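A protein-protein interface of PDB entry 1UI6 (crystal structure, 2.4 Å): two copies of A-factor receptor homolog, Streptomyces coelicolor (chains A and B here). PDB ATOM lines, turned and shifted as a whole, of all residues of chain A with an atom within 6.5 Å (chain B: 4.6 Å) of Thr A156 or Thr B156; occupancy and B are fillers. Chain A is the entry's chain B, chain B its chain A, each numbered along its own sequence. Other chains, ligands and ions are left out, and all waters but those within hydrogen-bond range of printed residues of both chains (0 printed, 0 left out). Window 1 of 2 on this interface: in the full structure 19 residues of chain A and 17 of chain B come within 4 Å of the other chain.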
ATOM      1  N   ASP A 151      42.236   6.070  17.768  1.00  0.00           N
ATOM      2  CA  ASP A 151      41.279   6.837  17.015  1.00  0.00           C
ATOM      3  C   ASP A 151      39.939   6.123  16.975  1.00  0.00           C
ATOM      4  O   ASP A 151      38.916   6.732  17.312  1.00  0.00           O
ATOM      5  CB  ASP A 151      41.819   7.176  15.635  1.00  0.00           C
ATOM      6  CG  ASP A 151      42.493   8.529  15.605  1.00  0.00           C
ATOM      7  OD1 ASP A 151      41.801   9.564  15.792  1.00  0.00           O
ATOM      8  OD2 ASP A 151      43.713   8.676  15.410  1.00  0.00           O
ATOM      9  N   SER A 152      39.957   4.831  16.644  1.00  0.00           N
ATOM     10  CA  SER A 152      38.743   4.023  16.580  1.00  0.00           C
ATOM     11  C   SER A 152      38.086   3.978  17.932  1.00  0.00           C
ATOM     12  O   SER A 152      36.881   3.996  18.021  1.00  0.00           O
ATOM     13  CB  SER A 152      39.053   2.575  16.203  1.00  0.00           C
ATOM     14  OG  SER A 152      39.774   2.488  14.994  1.00  0.00           O
ATOM     15  N   VAL A 153      38.881   3.864  18.984  1.00  0.00           N
ATOM     16  CA  VAL A 153      38.304   3.809  20.298  1.00  0.00           C
ATOM     17  C   VAL A 153      37.662   5.166  20.668  1.00  0.00           C
ATOM     18  O   VAL A 153      36.561   5.228  21.253  1.00  0.00           O
ATOM     19  CB  VAL A 153      39.346   3.403  21.367  1.00  0.00           C
ATOM     20  CG1 VAL A 153      38.711   3.375  22.722  1.00  0.00           C
ATOM     21  CG2 VAL A 153      39.925   2.059  21.076  1.00  0.00           C
ATOM     22  N   ALA A 154      38.341   6.251  20.309  1.00  0.00           N
ATOM     23  CA  ALA A 154      37.837   7.559  20.667  1.00  0.00           C
ATOM     24  C   ALA A 154      36.511   7.742  19.974  1.00  0.00           C
ATOM     25  O   ALA A 154      35.517   8.144  20.564  1.00  0.00           O
ATOM     26  CB  ALA A 154      38.814   8.616  20.264  1.00  0.00           C
ATOM     27  N   HIS A 155      36.499   7.360  18.712  1.00  0.00           N
ATOM     28  CA  HIS A 155      35.300   7.479  17.923  1.00  0.00           C
ATOM     29  C   HIS A 155      34.144   6.701  18.541  1.00  0.00           C
ATOM     30  O   HIS A 155      33.031   7.214  18.649  1.00  0.00           O
ATOM     31  CB  HIS A 155      35.546   6.979  16.528  1.00  0.00           C
ATOM     32  CG  HIS A 155      34.450   7.321  15.587  1.00  0.00           C
ATOM     33  ND1 HIS A 155      34.044   6.475  14.585  1.00  0.00           N
ATOM     34  CD2 HIS A 155      33.656   8.414  15.504  1.00  0.00           C
ATOM     35  CE1 HIS A 155      33.066   7.042  13.903  1.00  0.00           C
ATOM     36  NE2 HIS A 155      32.800   8.212  14.451  1.00  0.00           N
ATOM     37  N   THR A 156      34.419   5.471  18.952  1.00  0.00           N
ATOM     38  CA  THR A 156      33.403   4.645  19.566  1.00  0.00           C
ATOM     39  C   THR A 156      32.840   5.296  20.821  1.00  0.00           C
ATOM     40  O   THR A 156      31.643   5.279  21.053  1.00  0.00           O
ATOM     41  CB  THR A 156      34.002   3.271  19.935  1.00  0.00           C
ATOM     42  OG1 THR A 156      34.177   2.505  18.747  1.00  0.00           O
ATOM     43  CG2 THR A 156      33.039   2.447  20.704  1.00  0.00           C
ATOM     44  N   LEU A 157      33.737   5.861  21.619  1.00  0.00           N
ATOM     45  CA  LEU A 157      33.388   6.497  22.847  1.00  0.00           C
ATOM     46  C   LEU A 157      32.465   7.637  22.590  1.00  0.00           C
ATOM     47  O   LEU A 157      31.455   7.765  23.267  1.00  0.00           O
ATOM     48  CB  LEU A 157      34.650   6.956  23.588  1.00  0.00           C
ATOM     49  CG  LEU A 157      35.301   5.890  24.493  1.00  0.00           C
ATOM     50  CD1 LEU A 157      36.481   6.442  25.288  1.00  0.00           C
ATOM     51  CD2 LEU A 157      34.332   5.243  25.483  1.00  0.00           C
ATOM     52  N   VAL A 158      32.801   8.474  21.616  1.00  0.00           N
ATOM     53  CA  VAL A 158      32.017   9.668  21.328  1.00  0.00           C
ATOM     54  C   VAL A 158      30.654   9.206  20.864  1.00  0.00           C
ATOM     55  O   VAL A 158      29.624   9.656  21.343  1.00  0.00           O
ATOM     56  CB  VAL A 158      32.684  10.510  20.223  1.00  0.00           C
ATOM     57  CG1 VAL A 158      31.756  11.642  19.746  1.00  0.00           C
ATOM     58  CG2 VAL A 158      33.995  11.097  20.689  1.00  0.00           C
ATOM     59  N   CYS A 159      30.662   8.282  19.917  1.00  0.00           N
ATOM     60  CA  CYS A 159      29.439   7.705  19.423  1.00  0.00           C
ATOM     61  C   CYS A 159      28.625   6.973  20.477  1.00  0.00           C
ATOM     62  O   CYS A 159      27.419   6.891  20.350  1.00  0.00           O
ATOM     63  CB  CYS A 159      29.743   6.753  18.294  1.00  0.00           C
ATOM     64  SG  CYS A 159      29.821   7.665  16.789  1.00  0.00           S
ATOM     65  N   SER A 160      29.235   6.426  21.515  1.00  0.00           N
ATOM     66  CA  SER A 160      28.375   5.740  22.472  1.00  0.00           C
ATOM     67  C   SER A 160      27.520   6.745  23.251  1.00  0.00           C
ATOM     68  O   SER A 160      26.492   6.386  23.769  1.00  0.00           O
ATOM     69  CB  SER A 160      29.138   4.735  23.366  1.00  0.00           C
ATOM     70  OG  SER A 160      29.959   5.357  24.313  1.00  0.00           O
ATOM     71  N   VAL A 161      27.927   8.005  23.295  1.00  0.00           N
ATOM     72  CA  VAL A 161      27.156   9.058  23.962  1.00  0.00           C
ATOM     73  C   VAL A 161      26.212   9.801  22.998  1.00  0.00           C
ATOM     74  O   VAL A 161      25.042  10.033  23.306  1.00  0.00           O
ATOM     75  CB  VAL A 161      28.070  10.127  24.557  1.00  0.00           C
ATOM     76  CG1 VAL A 161      27.229  11.194  25.214  1.00  0.00           C
ATOM     77  CG2 VAL A 161      29.026   9.533  25.572  1.00  0.00           C
ATOM     78  N   VAL A 162      26.732  10.192  21.839  1.00  0.00           N
ATOM     79  CA  VAL A 162      25.922  10.852  20.815  1.00  0.00           C
ATOM     80  C   VAL A 162      24.815   9.940  20.280  1.00  0.00           C
ATOM     81  O   VAL A 162      25.099   8.830  19.811  1.00  0.00           O
ATOM     82  CB  VAL A 162      26.780  11.273  19.616  1.00  0.00           C
ATOM     83  CG1 VAL A 162      25.894  11.694  18.456  1.00  0.00           C
ATOM     84  CG2 VAL A 162      27.774  12.374  20.019  1.00  0.00           C
ATOM     85  N   ARG A 180      23.927   2.919  27.704  1.00  0.00           N
ATOM     86  CA  ARG A 180      24.609   2.728  26.452  1.00  0.00           C
ATOM     87  C   ARG A 180      26.071   3.003  26.589  1.00  0.00           C
ATOM     88  O   ARG A 180      26.889   2.373  25.916  1.00  0.00           O
ATOM     89  CB  ARG A 180      24.042   3.644  25.365  1.00  0.00           C
ATOM     90  CG  ARG A 180      22.640   3.276  24.851  1.00  0.00           C
ATOM     91  CD  ARG A 180      22.067   4.283  23.863  1.00  0.00           C
ATOM     92  NE  ARG A 180      20.877   3.778  23.181  1.00  0.00           N
ATOM     93  CZ  ARG A 180      19.650   3.765  23.688  1.00  0.00           C
ATOM     94  NH1 ARG A 180      19.420   4.218  24.903  1.00  0.00           N
ATOM     95  NH2 ARG A 180      18.637   3.290  22.980  1.00  0.00           N
ATOM     96  N   LEU A 181      26.409   3.963  27.438  1.00  0.00           N
ATOM     97  CA  LEU A 181      27.814   4.328  27.610  1.00  0.00           C
ATOM     98  C   LEU A 181      28.521   3.200  28.415  1.00  0.00           C
ATOM     99  O   LEU A 181      29.643   2.796  28.119  1.00  0.00           O
ATOM    100  CB  LEU A 181      27.904   5.687  28.275  1.00  0.00           C
ATOM    101  CG  LEU A 181      29.291   6.220  28.578  1.00  0.00           C
ATOM    102  CD1 LEU A 181      30.210   6.253  27.318  1.00  0.00           C
ATOM    103  CD2 LEU A 181      29.163   7.566  29.188  1.00  0.00           C
ATOM    104  N   MET A 184      28.944  -0.018  26.182  1.00  0.00           N
ATOM    105  CA  MET A 184      30.078   0.158  25.305  1.00  0.00           C
ATOM    106  C   MET A 184      31.408   0.114  26.065  1.00  0.00           C
ATOM    107  O   MET A 184      32.395  -0.378  25.541  1.00  0.00           O
ATOM    108  CB  MET A 184      29.901   1.442  24.528  1.00  0.00           C
ATOM    109  CG  MET A 184      28.979   1.230  23.316  1.00  0.00           C
ATOM    110  SD  MET A 184      29.288  -0.376  22.444  1.00  0.00           S
ATOM    111  CE  MET A 184      31.052  -0.187  22.089  1.00  0.00           C
ATOM    112  N   LEU A 188      34.675  -2.310  25.359  1.00  0.00           N
ATOM    113  CA  LEU A 188      36.023  -1.773  25.163  1.00  0.00           C
ATOM    114  C   LEU A 188      37.009  -2.349  26.171  1.00  0.00           C
ATOM    115  O   LEU A 188      38.119  -2.694  25.799  1.00  0.00           O
ATOM    116  CB  LEU A 188      36.055  -0.234  25.251  1.00  0.00           C
ATOM    117  CG  LEU A 188      35.366   0.510  24.121  1.00  0.00           C
ATOM    118  CD1 LEU A 188      35.339   1.998  24.410  1.00  0.00           C
ATOM    119  CD2 LEU A 188      36.088   0.261  22.849  1.00  0.00           C
ATOM    120  N   SER B 152      22.139  -1.123  22.675  1.00  0.00           N
ATOM    121  CA  SER B 152      23.182  -0.136  22.854  1.00  0.00           C
ATOM    122  C   SER B 152      24.234  -0.229  21.781  1.00  0.00           C
ATOM    123  O   SER B 152      24.632   0.772  21.226  1.00  0.00           O
ATOM    124  CB  SER B 152      23.788  -0.249  24.247  1.00  0.00           C
ATOM    125  OG  SER B 152      25.136   0.219  24.278  1.00  0.00           O
ATOM    126  N   VAL B 153      24.690  -1.427  21.466  1.00  0.00           N
ATOM    127  CA  VAL B 153      25.662  -1.602  20.373  1.00  0.00           C
ATOM    128  C   VAL B 153      25.099  -1.245  18.981  1.00  0.00           C
ATOM    129  O   VAL B 153      25.834  -0.808  18.084  1.00  0.00           O
ATOM    130  CB  VAL B 153      26.136  -3.041  20.307  1.00  0.00           C
ATOM    131  CG1 VAL B 153      27.229  -3.196  19.297  1.00  0.00           C
ATOM    132  CG2 VAL B 153      26.640  -3.482  21.651  1.00  0.00           C
ATOM    133  N   ALA B 154      23.812  -1.471  18.765  1.00  0.00           N
ATOM    134  CA  ALA B 154      23.244  -1.093  17.483  1.00  0.00           C
ATOM    135  C   ALA B 154      23.337   0.435  17.374  1.00  0.00           C
ATOM    136  O   ALA B 154      23.860   0.973  16.386  1.00  0.00           O
ATOM    137  CB  ALA B 154      21.832  -1.549  17.378  1.00  0.00           C
ATOM    138  N   HIS B 155      22.879   1.103  18.435  1.00  0.00           N
ATOM    139  CA  HIS B 155      22.872   2.559  18.493  1.00  0.00           C
ATOM    140  C   HIS B 155      24.231   3.152  18.263  1.00  0.00           C
ATOM    141  O   HIS B 155      24.381   4.156  17.544  1.00  0.00           O
ATOM    142  CB  HIS B 155      22.356   3.051  19.837  1.00  0.00           C
ATOM    143  CG  HIS B 155      20.876   3.228  19.872  1.00  0.00           C
ATOM    144  ND1 HIS B 155      20.256   4.366  19.406  1.00  0.00           N
ATOM    145  CD2 HIS B 155      19.894   2.399  20.286  1.00  0.00           C
ATOM    146  CE1 HIS B 155      18.949   4.232  19.543  1.00  0.00           C
ATOM    147  NE2 HIS B 155      18.703   3.048  20.075  1.00  0.00           N
ATOM    148  N   THR B 156      25.221   2.531  18.886  1.00  0.00           N
ATOM    149  CA  THR B 156      26.576   3.005  18.757  1.00  0.00           C
ATOM    150  C   THR B 156      27.098   2.617  17.395  1.00  0.00           C
ATOM    151  O   THR B 156      27.723   3.426  16.736  1.00  0.00           O
ATOM    152  CB  THR B 156      27.485   2.477  19.906  1.00  0.00           C
ATOM    153  OG1 THR B 156      27.142   3.107  21.159  1.00  0.00           O
ATOM    154  CG2 THR B 156      28.935   2.901  19.681  1.00  0.00           C
ATOM    155  N   LEU B 157      26.839   1.385  16.971  1.00  0.00           N
ATOM    156  CA  LEU B 157      27.350   0.898  15.685  1.00  0.00           C
ATOM    157  C   LEU B 157      26.899   1.824  14.562  1.00  0.00           C
ATOM    158  O   LEU B 157      27.701   2.275  13.786  1.00  0.00           O
ATOM    159  CB  LEU B 157      26.900  -0.554  15.440  1.00  0.00           C
ATOM    160  CG  LEU B 157      27.252  -1.269  14.127  1.00  0.00           C
ATOM    161  CD1 LEU B 157      28.707  -1.113  13.783  1.00  0.00           C
ATOM    162  CD2 LEU B 157      26.923  -2.748  14.191  1.00  0.00           C
ATOM    163  N   VAL B 158      25.613   2.134  14.502  1.00  0.00           N
ATOM    164  CA  VAL B 158      25.129   3.045  13.477  1.00  0.00           C
ATOM    165  C   VAL B 158      25.939   4.348  13.503  1.00  0.00           C
ATOM    166  O   VAL B 158      26.524   4.739  12.494  1.00  0.00           O
ATOM    167  CB  VAL B 158      23.609   3.277  13.597  1.00  0.00           C
ATOM    168  CG1 VAL B 158      23.148   4.374  12.648  1.00  0.00           C
ATOM    169  CG2 VAL B 158      22.871   1.980  13.268  1.00  0.00           C
ATOM    170  N   CYS B 159      25.998   5.003  14.650  1.00  0.00           N
ATOM    171  CA  CYS B 159      26.820   6.195  14.777  1.00  0.00           C
ATOM    172  C   CYS B 159      28.261   5.923  14.344  1.00  0.00           C
ATOM    173  O   CYS B 159      28.879   6.741  13.706  1.00  0.00           O
ATOM    174  CB  CYS B 159      26.826   6.751  16.200  1.00  0.00           C
ATOM    175  SG  CYS B 159      27.836   8.242  16.381  1.00  0.00           S
ATOM    176  N   SER B 160      28.804   4.778  14.679  1.00  0.00           N
ATOM    177  CA  SER B 160      30.208   4.497  14.345  1.00  0.00           C
ATOM    178  C   SER B 160      30.490   4.310  12.854  1.00  0.00           C
ATOM    179  O   SER B 160      31.525   4.739  12.353  1.00  0.00           O
ATOM    180  CB  SER B 160      30.689   3.284  15.133  1.00  0.00           C
ATOM    181  OG  SER B 160      30.570   3.558  16.515  1.00  0.00           O
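The side-chain sulfur of Cys B159 forms a disulfide with the side-chain sulfur of Cys A159, at 2.1 Å. N of Ser B160 sits at hydrogen-bond distance from SG of Cys A159. The guanidinium group (NH2) of Arg A180 is in hydrogen-bond range of a ring nitrogen (NE2) of His B155 (2.9 Å). The side-chain hydroxyl (OG) of Ser B152 lies within hydrogen-bond range of the backbone carbonyl oxygen (O) of Arg A180 (3.2 Å).
The side-chain hydroxyl of Thr B156 is in hydrogen-bond range of the backbone carbonyl oxygen of Ser B152, 3.4 Å away. The side-chain hydroxyl (OG) of Ser B160 sits at hydrogen-bond distance from the backbone carbonyl oxygen (O) of Thr B156 (2.9 Å). O of Leu A157 is in hydrogen-bond range of OG of Ser A160. The backbone carbonyl oxygen (O) of Ser A152 sits at hydrogen-bond distance from the side-chain hydroxyl (OG1) of Thr A156, at 3.2 Å.
Among the printed residues, pairs that only touch across the chains: His A155 with Ser B160 (3.2 Å), Thr A156 with Thr B156 (3.9 Å), Cys A159 with Thr B156 (3.9 Å), Ser A160 with Thr B156 (3.2 Å) and Met A184 with Thr B156 (3.4 Å).
Thr B156 touches just these residues of chain A: Thr A156 (3.9 Å), Cys A159 (3.9 Å), Ser A160 (3.2 Å) and Met A184 (3.4 Å). Printed residues of chain B within 4 Å of His A155: Ser B160 (3.2 Å). Of the printed residues of chain A, Ser B152 touches Arg A180 (3.2 Å). The nearest residue of chain A that does not touch Thr B156 is Arg A180 (4.8 Å).
Of the 16 printed residues of chain A, 6 touch a printed residue of chain B. Hydrophobic or aromatic side chains of chain B that line the printed part of chain A: His B155. Among the printed residues, 9 pairs touch across the chains.
Thr A156 touches its own counterpart, Thr B156. Cys A159 touches Thr B156, but with the chains exchanged Thr A156 does not touch Cys B159 (6.7 Å). Cys A159 touches its own counterpart, Cys B159. Ser A160 touches Thr B156, but with the chains exchanged Thr A156 does not touch Ser B160 (4.3 Å).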
